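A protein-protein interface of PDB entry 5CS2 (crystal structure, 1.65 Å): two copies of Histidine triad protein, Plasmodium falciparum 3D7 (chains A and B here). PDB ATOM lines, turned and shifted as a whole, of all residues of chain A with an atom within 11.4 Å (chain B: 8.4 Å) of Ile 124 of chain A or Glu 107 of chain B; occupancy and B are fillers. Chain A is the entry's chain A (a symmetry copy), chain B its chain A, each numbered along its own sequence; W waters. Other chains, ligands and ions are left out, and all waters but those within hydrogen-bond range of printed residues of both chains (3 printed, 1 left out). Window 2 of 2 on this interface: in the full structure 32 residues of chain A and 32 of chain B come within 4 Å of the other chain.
O of Gly 109 of chain B is in hydrogen-bond range of NE2 of Gln 103 of chain B (3.3 Å). The backbone NH of Gln 110 of chain B lies within hydrogen-bond range of the backbone carbonyl oxygen of Gly 105 of chain B, 3.2 Å away. The backbone carbonyl oxygen (O) of Phe 93 of chain A sits at hydrogen-bond distance from the side-chain amino group (NZ) of Lys 123 of chain A (2.8 Å). The backbone carbonyl oxygen (O) of Asp 97 of chain A sits at hydrogen-bond distance from the backbone NH (N) of Arg 122 of chain A (2.8 Å). The side-chain hydroxyl of Thr 95 of chain A lies within hydrogen-bond range of the backbone carbonyl oxygen of Arg 122 of chain A (2.7 Å). The side-chain carboxylate (OD1) of Asp 104 of chain B lies within hydrogen-bond range of a ring nitrogen (ND1) of His 66 of chain B (3.1 Å).
Of chain B, only Glu 107 comes within 4 Å of Ile 124 of chain A. Of the printed residues of chain A, Glu 107 of chain B touches Asp 97, Arg 122, Lys 123 and Ile 124. Asn 125 of chain A touches none of the printed residues of chain B. Gly 105 of chain B touches just one residue of chain A: Asp 97 (3.4 Å). Lys 106 of chain B touches just one residue of chain A: Asp 97. Ala 108 of chain B touches just these residues of chain A: Phe 98 (3.2 Å), Ser 99 (3.8 Å) and Arg 122 (3.96 Å). Of the printed residues of chain B, Arg 122 of chain A touches Glu 107 and Ala 108. Of the printed residues of chain B, Thr 96 of chain A touches His 66 and Asp 104. Of the printed residues of chain A, Asp 104 of chain B touches Thr 96 (3.7 Å), Asp 97 (3.1 Å) and Phe 98 (2.9 Å). Of the printed residues of chain A, His 66 of chain B touches Thr 96 (3.2 Å) and Asp 97 (3.3 Å). The nearest printed residue of chain B that does not touch Lys 123 of chain A is Ala 108 of chain B (6.4 Å).
Water W1 bridges OE2 of Glu 107 of chain B and N of Asn 125 of chain A. Water W3 lies within hydrogen-bond range of OG of Ser 99 of chain A and O of Ala 108 of chain B. Water W2 lies within hydrogen-bond range of OD1 of Asp 97 of chain A, N of Lys 106 of chain B and NE2 of His 66 of chain B.
No position is printed for both chains. Of the 15 pairs that touch across the chains among the printed residues, none has its exchanged pair printed and touching as well.
Hydrophobic or aromatic side chains of chain A that line the printed part of chain B: Phe 98 and Ile 124. Of the 10 printed residues of chain B, 7 touch a printed residue of chain A.
Among the printed residues, pairs that only touch across the chains: Asp 97 of chain A with Asp 104 of chain B, Phe 98 of chain A with Ala 108 of chain B, Asp 97 of chain A with His 66 of chain B, Asp 97 of chain A with Gly 105 of chain B, Ile 124 of chain A with Glu 107 of chain B, Arg 122 of chain A with Glu 107 of chain B, Thr 96 of chain A with Asp 104 of chain B, Ser 99 of chain A with Ala 108 of chain B, Arg 122 of chain A with Ala 108 of chain B, Phe 98 of chain A with Gln 103 of chain B and Lys 123 of chain A with Glu 107 of chain B.
A ring nitrogen (ND1) of His 66 of chain B sits close to the backbone carbonyl oxygen (O) of Thr 96 of chain A, at 3.3 Å. The side-chain carboxylate of Asp 97 of chain A lies within hydrogen-bond range of the backbone NH of Lys 106 of chain B (3.4 Å). The backbone NH (N) of Glu 107 of chain B sits at hydrogen-bond distance from the side-chain carboxylate (OD2) of Asp 97 of chain A (2.8 Å). The backbone carbonyl oxygen (O) of Phe 98 of chain A lies within hydrogen-bond range of the backbone NH (N) of Asp 104 of chain B, at 2.9 Å.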
ATOM      1  N   LEU A  52     -21.522  17.659 -29.042  1.00  0.00           N
ATOM      2  CA  LEU A  52     -21.646  19.084 -29.325  1.00  0.00           C
ATOM      3  C   LEU A  52     -21.390  19.281 -30.816  1.00  0.00           C
ATOM      4  O   LEU A  52     -20.783  18.392 -31.426  1.00  0.00           O
ATOM      5  CB  LEU A  52     -20.571  19.872 -28.540  1.00  0.00           C
ATOM      6  CG  LEU A  52     -20.696  19.947 -27.015  1.00  0.00           C
ATOM      7  CD1 LEU A  52     -19.451  20.609 -26.423  1.00  0.00           C
ATOM      8  CD2 LEU A  52     -21.930  20.738 -26.587  1.00  0.00           C
ATOM      9  N   PRO A  53     -21.731  20.456 -31.421  1.00  0.00           N
ATOM     10  CA  PRO A  53     -21.445  20.649 -32.866  1.00  0.00           C
ATOM     11  C   PRO A  53     -19.970  20.551 -33.244  1.00  0.00           C
ATOM     12  O   PRO A  53     -19.103  21.041 -32.535  1.00  0.00           O
ATOM     13  CB  PRO A  53     -21.970  22.063 -33.156  1.00  0.00           C
ATOM     14  CG  PRO A  53     -22.907  22.372 -32.059  1.00  0.00           C
ATOM     15  CD  PRO A  53     -22.446  21.621 -30.853  1.00  0.00           C
ATOM     16  N   PHE A  93     -15.210  26.269 -37.017  1.00  0.00           N
ATOM     17  CA  PHE A  93     -16.163  26.464 -35.930  1.00  0.00           C
ATOM     18  C   PHE A  93     -15.878  27.722 -35.101  1.00  0.00           C
ATOM     19  O   PHE A  93     -16.598  27.993 -34.146  1.00  0.00           O
ATOM     20  CB  PHE A  93     -16.252  25.184 -35.058  1.00  0.00           C
ATOM     21  CG  PHE A  93     -17.093  24.136 -35.757  1.00  0.00           C
ATOM     22  CD1 PHE A  93     -16.557  23.358 -36.782  1.00  0.00           C
ATOM     23  CD2 PHE A  93     -18.446  24.003 -35.466  1.00  0.00           C
ATOM     24  CE1 PHE A  93     -17.363  22.460 -37.495  1.00  0.00           C
ATOM     25  CE2 PHE A  93     -19.246  23.098 -36.176  1.00  0.00           C
ATOM     26  CZ  PHE A  93     -18.694  22.330 -37.182  1.00  0.00           C
ATOM     27  N   ASN A  94     -14.889  28.518 -35.513  1.00  0.00           N
ATOM     28  CA  ASN A  94     -14.445  29.771 -34.882  1.00  0.00           C
ATOM     29  C   ASN A  94     -14.165  29.578 -33.380  1.00  0.00           C
ATOM     30  O   ASN A  94     -14.855  30.118 -32.501  1.00  0.00           O
ATOM     31  CB  ASN A  94     -15.412  30.930 -35.192  1.00  0.00           C
ATOM     32  CG  ASN A  94     -15.563  31.160 -36.678  1.00  0.00           C
ATOM     33  OD1 ASN A  94     -14.578  31.258 -37.428  1.00  0.00           O
ATOM     34  ND2 ASN A  94     -16.796  31.161 -37.151  1.00  0.00           N
ATOM     35  N   THR A  95     -13.186  28.707 -33.101  1.00  0.00           N
ATOM     36  CA  THR A  95     -12.785  28.423 -31.728  1.00  0.00           C
ATOM     37  C   THR A  95     -11.342  28.053 -31.659  1.00  0.00           C
ATOM     38  O   THR A  95     -10.740  27.594 -32.635  1.00  0.00           O
ATOM     39  CB  THR A  95     -13.694  27.389 -31.007  1.00  0.00           C
ATOM     40  OG1 THR A  95     -13.332  27.366 -29.614  1.00  0.00           O
ATOM     41  CG2 THR A  95     -13.580  25.967 -31.601  1.00  0.00           C
ATOM     42  N   THR A  96     -10.777  28.265 -30.486  1.00  0.00           N
ATOM     43  CA  THR A  96      -9.397  27.915 -30.263  1.00  0.00           C
ATOM     44  C   THR A  96      -9.386  26.733 -29.267  1.00  0.00           C
ATOM     45  O   THR A  96      -8.312  26.224 -28.983  1.00  0.00           O
ATOM     46  CB  THR A  96      -8.659  29.124 -29.649  1.00  0.00           C
ATOM     47  OG1 THR A  96      -9.259  29.435 -28.388  1.00  0.00           O
ATOM     48  CG2 THR A  96      -8.690  30.364 -30.574  1.00  0.00           C
ATOM     49  N   ASP A  97     -10.551  26.382 -28.678  1.00  0.00           N
ATOM     50  CA  ASP A  97     -10.621  25.375 -27.613  1.00  0.00           C
ATOM     51  C   ASP A  97     -11.260  24.064 -28.025  1.00  0.00           C
ATOM     52  O   ASP A  97     -12.284  24.052 -28.710  1.00  0.00           O
ATOM     53  CB  ASP A  97     -11.331  25.929 -26.378  1.00  0.00           C
ATOM     54  CG  ASP A  97     -10.719  27.199 -25.793  1.00  0.00           C
ATOM     55  OD1 ASP A  97      -9.593  27.584 -26.228  1.00  0.00           O
ATOM     56  OD2 ASP A  97     -11.347  27.792 -24.887  1.00  0.00           O
ATOM     57  N   PHE A  98     -10.639  22.945 -27.590  1.00  0.00           N
ATOM     58  CA  PHE A  98     -11.101  21.609 -27.969  1.00  0.00           C
ATOM     59  C   PHE A  98     -10.938  20.646 -26.820  1.00  0.00           C
ATOM     60  O   PHE A  98      -9.994  20.779 -26.038  1.00  0.00           O
ATOM     61  CB  PHE A  98     -10.243  21.046 -29.132  1.00  0.00           C
ATOM     62  CG  PHE A  98     -10.199  21.924 -30.352  1.00  0.00           C
ATOM     63  CD1 PHE A  98     -11.178  21.816 -31.337  1.00  0.00           C
ATOM     64  CD2 PHE A  98      -9.256  22.931 -30.465  1.00  0.00           C
ATOM     65  CE1 PHE A  98     -11.193  22.688 -32.423  1.00  0.00           C
ATOM     66  CE2 PHE A  98      -9.270  23.806 -31.556  1.00  0.00           C
ATOM     67  CZ  PHE A  98     -10.236  23.671 -32.523  1.00  0.00           C
ATOM     68  N   SER A  99     -11.824  19.671 -26.753  1.00  0.00           N
ATOM     69  CA  SER A  99     -11.693  18.516 -25.860  1.00  0.00           C
ATOM     70  C   SER A  99     -11.184  17.415 -26.791  1.00  0.00           C
ATOM     71  O   SER A  99     -11.772  17.159 -27.858  1.00  0.00           O
ATOM     72  CB  SER A  99     -13.021  18.102 -25.234  1.00  0.00           C
ATOM     73  OG  SER A  99     -13.495  19.070 -24.319  1.00  0.00           O
ATOM     74  N   ILE A 100     -10.026  16.849 -26.462  1.00  0.00           N
ATOM     75  CA  ILE A 100      -9.429  15.812 -27.289  1.00  0.00           C
ATOM     76  C   ILE A 100      -9.332  14.577 -26.417  1.00  0.00           C
ATOM     77  O   ILE A 100      -8.813  14.676 -25.303  1.00  0.00           O
ATOM     78  CB  ILE A 100      -8.062  16.234 -27.854  1.00  0.00           C
ATOM     79  CG1 ILE A 100      -8.130  17.629 -28.585  1.00  0.00           C
ATOM     80  CG2 ILE A 100      -7.474  15.125 -28.738  1.00  0.00           C
ATOM     81  CD1 ILE A 100      -6.748  18.222 -28.726  1.00  0.00           C
ATOM     82  N   ILE A 120     -13.622  17.530 -30.019  1.00  0.00           N
ATOM     83  CA  ILE A 120     -14.878  18.264 -29.788  1.00  0.00           C
ATOM     84  C   ILE A 120     -14.574  19.742 -29.634  1.00  0.00           C
ATOM     85  O   ILE A 120     -14.015  20.168 -28.611  1.00  0.00           O
ATOM     86  CB  ILE A 120     -15.720  17.730 -28.595  1.00  0.00           C
ATOM     87  CG1 ILE A 120     -15.909  16.194 -28.635  1.00  0.00           C
ATOM     88  CG2 ILE A 120     -17.086  18.464 -28.521  1.00  0.00           C
ATOM     89  CD1 ILE A 120     -16.097  15.522 -27.298  1.00  0.00           C
ATOM     90  N   PRO A 121     -15.018  20.570 -30.588  1.00  0.00           N
ATOM     91  CA  PRO A 121     -14.808  22.024 -30.451  1.00  0.00           C
ATOM     92  C   PRO A 121     -15.562  22.510 -29.225  1.00  0.00           C
ATOM     93  O   PRO A 121     -16.630  21.980 -28.915  1.00  0.00           O
ATOM     94  CB  PRO A 121     -15.428  22.590 -31.738  1.00  0.00           C
ATOM     95  CG  PRO A 121     -15.407  21.436 -32.707  1.00  0.00           C
ATOM     96  CD  PRO A 121     -15.734  20.252 -31.840  1.00  0.00           C
ATOM     97  N   ARG A 122     -14.981  23.462 -28.481  1.00  0.00           N
ATOM     98  CA  ARG A 122     -15.600  23.959 -27.245  1.00  0.00           C
ATOM     99  C   ARG A 122     -15.817  25.482 -27.249  1.00  0.00           C
ATOM    100  O   ARG A 122     -14.970  26.221 -27.742  1.00  0.00           O
ATOM    101  CB  ARG A 122     -14.734  23.581 -26.032  1.00  0.00           C
ATOM    102  CG  ARG A 122     -14.521  22.074 -25.810  1.00  0.00           C
ATOM    103  CD  ARG A 122     -15.806  21.287 -25.731  1.00  0.00           C
ATOM    104  NE  ARG A 122     -16.673  21.737 -24.641  1.00  0.00           N
ATOM    105  CZ  ARG A 122     -16.579  21.303 -23.388  1.00  0.00           C
ATOM    106  NH1 ARG A 122     -15.671  20.391 -23.059  1.00  0.00           N
ATOM    107  NH2 ARG A 122     -17.399  21.773 -22.455  1.00  0.00           N
ATOM    108  N   LYS A 123     -16.958  25.931 -26.680  1.00  0.00           N
ATOM    109  CA  LYS A 123     -17.361  27.345 -26.546  1.00  0.00           C
ATOM    110  C   LYS A 123     -17.940  27.624 -25.150  1.00  0.00           C
ATOM    111  O   LYS A 123     -18.327  26.684 -24.453  1.00  0.00           O
ATOM    112  CB  LYS A 123     -18.369  27.715 -27.649  1.00  0.00           C
ATOM    113  CG  LYS A 123     -17.726  27.835 -29.023  1.00  0.00           C
ATOM    114  CD  LYS A 123     -18.717  27.585 -30.155  1.00  0.00           C
ATOM    115  CE  LYS A 123     -18.222  28.232 -31.428  1.00  0.00           C
ATOM    116  NZ  LYS A 123     -18.961  27.769 -32.634  1.00  0.00           N
ATOM    117  N   ILE A 124     -17.986  28.906 -24.725  1.00  0.00           N
ATOM    118  CA  ILE A 124     -18.522  29.294 -23.400  1.00  0.00           C
ATOM    119  C   ILE A 124     -19.933  28.736 -23.159  1.00  0.00           C
ATOM    120  O   ILE A 124     -20.820  28.877 -24.011  1.00  0.00           O
ATOM    121  CB  ILE A 124     -18.456  30.834 -23.137  1.00  0.00           C
ATOM    122  CG1 ILE A 124     -17.023  31.380 -23.301  1.00  0.00           C
ATOM    123  CG2 ILE A 124     -19.051  31.217 -21.749  1.00  0.00           C
ATOM    124  CD1 ILE A 124     -16.904  32.920 -23.506  1.00  0.00           C
ATOM    125  N   ASN A 125     -20.111  28.072 -22.000  1.00  0.00           N
ATOM    126  CA  ASN A 125     -21.359  27.476 -21.516  1.00  0.00           C
ATOM    127  C   ASN A 125     -22.046  26.538 -22.536  1.00  0.00           C
ATOM    128  O   ASN A 125     -23.286  26.478 -22.575  1.00  0.00           O
ATOM    129  CB  ASN A 125     -22.332  28.575 -21.002  1.00  0.00           C
ATOM    130  CG  ASN A 125     -21.879  29.308 -19.753  1.00  0.00           C
ATOM    131  OD1 ASN A 125     -21.017  28.844 -18.985  1.00  0.00           O
ATOM    132  ND2 ASN A 125     -22.491  30.457 -19.493  1.00  0.00           N
ATOM    133  N   ASP A 126     -21.243  25.795 -23.345  1.00  0.00           N
ATOM    134  CA  ASP A 126     -21.772  24.838 -24.321  1.00  0.00           C
ATOM    135  C   ASP A 126     -22.307  23.603 -23.610  1.00  0.00           C
ATOM    136  O   ASP A 126     -23.415  23.174 -23.899  1.00  0.00           O
ATOM    137  CB  ASP A 126     -20.707  24.445 -25.367  1.00  0.00           C
ATOM    138  CG  ASP A 126     -19.377  23.883 -24.863  1.00  0.00           C
ATOM    139  OD1 ASP A 126     -19.272  23.574 -23.655  1.00  0.00           O
ATOM    140  OD2 ASP A 126     -18.434  23.788 -25.673  1.00  0.00           O
ATOM    141  N   HIS B  66      -1.586  26.177 -26.294  1.00  0.00           N
ATOM    142  CA  HIS B  66      -2.489  25.353 -27.080  1.00  0.00           C
ATOM    143  C   HIS B  66      -1.780  24.240 -27.804  1.00  0.00           C
ATOM    144  O   HIS B  66      -0.645  24.390 -28.218  1.00  0.00           O
ATOM    145  CB  HIS B  66      -3.252  26.222 -28.093  1.00  0.00           C
ATOM    146  CG  HIS B  66      -4.423  26.930 -27.484  1.00  0.00           C
ATOM    147  ND1 HIS B  66      -5.591  26.245 -27.150  1.00  0.00           N
ATOM    148  CD2 HIS B  66      -4.567  28.234 -27.158  1.00  0.00           C
ATOM    149  CE1 HIS B  66      -6.388  27.151 -26.610  1.00  0.00           C
ATOM    150  NE2 HIS B  66      -5.816  28.364 -26.601  1.00  0.00           N
ATOM    151  N   GLN B 103      -7.241  18.851 -22.372  1.00  0.00           N
ATOM    152  CA  GLN B 103      -8.232  19.920 -22.207  1.00  0.00           C
ATOM    153  C   GLN B 103      -7.545  21.080 -22.919  1.00  0.00           C
ATOM    154  O   GLN B 103      -6.736  21.797 -22.323  1.00  0.00           O
ATOM    155  CB  GLN B 103      -8.476  20.240 -20.712  1.00  0.00           C
ATOM    156  CG  GLN B 103      -8.977  19.051 -19.924  1.00  0.00           C
ATOM    157  CD  GLN B 103      -8.866  19.333 -18.455  1.00  0.00           C
ATOM    158  OE1 GLN B 103      -7.775  19.445 -17.902  1.00  0.00           O
ATOM    159  NE2 GLN B 103      -9.995  19.513 -17.818  1.00  0.00           N
ATOM    160  N   ASP B 104      -7.755  21.179 -24.241  1.00  0.00           N
ATOM    161  CA  ASP B 104      -7.071  22.155 -25.074  1.00  0.00           C
ATOM    162  C   ASP B 104      -7.743  23.530 -25.060  1.00  0.00           C
ATOM    163  O   ASP B 104      -8.371  23.925 -26.037  1.00  0.00           O
ATOM    164  CB  ASP B 104      -6.899  21.602 -26.495  1.00  0.00           C
ATOM    165  CG  ASP B 104      -6.091  22.458 -27.437  1.00  0.00           C
ATOM    166  OD1 ASP B 104      -5.205  23.210 -26.953  1.00  0.00           O
ATOM    167  OD2 ASP B 104      -6.257  22.298 -28.666  1.00  0.00           O
ATOM    168  N   GLY B 105      -7.570  24.257 -23.968  1.00  0.00           N
ATOM    169  CA  GLY B 105      -8.135  25.595 -23.850  1.00  0.00           C
ATOM    170  C   GLY B 105      -9.073  25.759 -22.683  1.00  0.00           C
ATOM    171  O   GLY B 105      -9.641  24.785 -22.180  1.00  0.00           O
ATOM    172  N   LYS B 106      -9.294  27.020 -22.267  1.00  0.00           N
ATOM    173  CA  LYS B 106     -10.127  27.334 -21.119  1.00  0.00           C
ATOM    174  C   LYS B 106     -11.545  26.757 -21.195  1.00  0.00           C
ATOM    175  O   LYS B 106     -12.060  26.246 -20.190  1.00  0.00           O
ATOM    176  CB  LYS B 106     -10.163  28.867 -20.867  1.00  0.00           C
ATOM    177  CG  LYS B 106     -10.574  29.242 -19.450  1.00  0.00           C
ATOM    178  CD  LYS B 106     -10.212  30.694 -19.105  1.00  0.00           C
ATOM    179  CE  LYS B 106     -10.140  30.935 -17.610  1.00  0.00           C
ATOM    180  NZ  LYS B 106      -8.977  30.246 -16.978  1.00  0.00           N
ATOM    181  N   GLU B 107     -12.175  26.817 -22.383  1.00  0.00           N
ATOM    182  CA  GLU B 107     -13.545  26.313 -22.502  1.00  0.00           C
ATOM    183  C   GLU B 107     -13.597  24.764 -22.543  1.00  0.00           C
ATOM    184  O   GLU B 107     -14.672  24.183 -22.407  1.00  0.00           O
ATOM    185  CB  GLU B 107     -14.294  27.001 -23.652  1.00  0.00           C
ATOM    186  CG  GLU B 107     -14.348  28.516 -23.413  1.00  0.00           C
ATOM    187  CD  GLU B 107     -14.759  28.966 -22.013  1.00  0.00           C
ATOM    188  OE1 GLU B 107     -14.113  29.885 -21.456  1.00  0.00           O
ATOM    189  OE2 GLU B 107     -15.718  28.382 -21.459  1.00  0.00           O
ATOM    190  N   ALA B 108     -12.416  24.116 -22.615  1.00  0.00           N
ATOM    191  CA  ALA B 108     -12.319  22.660 -22.470  1.00  0.00           C
ATOM    192  C   ALA B 108     -11.914  22.277 -21.019  1.00  0.00           C
ATOM    193  O   ALA B 108     -11.711  21.093 -20.716  1.00  0.00           O
ATOM    194  CB  ALA B 108     -11.331  22.096 -23.465  1.00  0.00           C
ATOM    195  N   GLY B 109     -11.866  23.271 -20.124  1.00  0.00           N
ATOM    196  CA  GLY B 109     -11.541  23.039 -18.715  1.00  0.00           C
ATOM    197  C   GLY B 109     -10.071  23.115 -18.337  1.00  0.00           C
ATOM    198  O   GLY B 109      -9.706  22.709 -17.230  1.00  0.00           O
ATOM    199  N   GLN B 110      -9.218  23.626 -19.217  1.00  0.00           N
ATOM    200  CA  GLN B 110      -7.780  23.763 -18.927  1.00  0.00           C
ATOM    201  C   GLN B 110      -7.592  24.786 -17.770  1.00  0.00           C
ATOM    202  O   GLN B 110      -8.153  25.884 -17.847  1.00  0.00           O
ATOM    203  CB  GLN B 110      -7.062  24.250 -20.189  1.00  0.00           C
ATOM    204  CG  GLN B 110      -5.548  24.270 -20.125  1.00  0.00           C
ATOM    205  CD  GLN B 110      -4.944  24.990 -21.301  1.00  0.00           C
ATOM    206  OE1 GLN B 110      -5.449  26.019 -21.763  1.00  0.00           O
ATOM    207  NE2 GLN B 110      -3.823  24.501 -21.791  1.00  0.00           N
ATOM    208  N   THR B 111      -6.883  24.399 -16.678  1.00  0.00           N
ATOM    209  CA  THR B 111      -6.648  25.306 -15.519  1.00  0.00           C
ATOM    210  C   THR B 111      -5.219  25.843 -15.484  1.00  0.00           C
ATOM    211  O   THR B 111      -4.960  26.877 -14.862  1.00  0.00           O
ATOM    212  CB  THR B 111      -7.030  24.680 -14.169  1.00  0.00           C
ATOM    213  OG1 THR B 111      -6.556  23.342 -14.080  1.00  0.00           O
ATOM    214  CG2 THR B 111      -8.517  24.756 -13.887  1.00  0.00           C
HETATM  215  O   HOH W   1     -17.734  27.094 -20.366  1.00  0.00           O
HETATM  216  O   HOH W   2      -8.175  28.985 -24.293  1.00  0.00           O
HETATM  217  O   HOH W   3     -12.285  18.774 -21.987  1.00  0.00           O
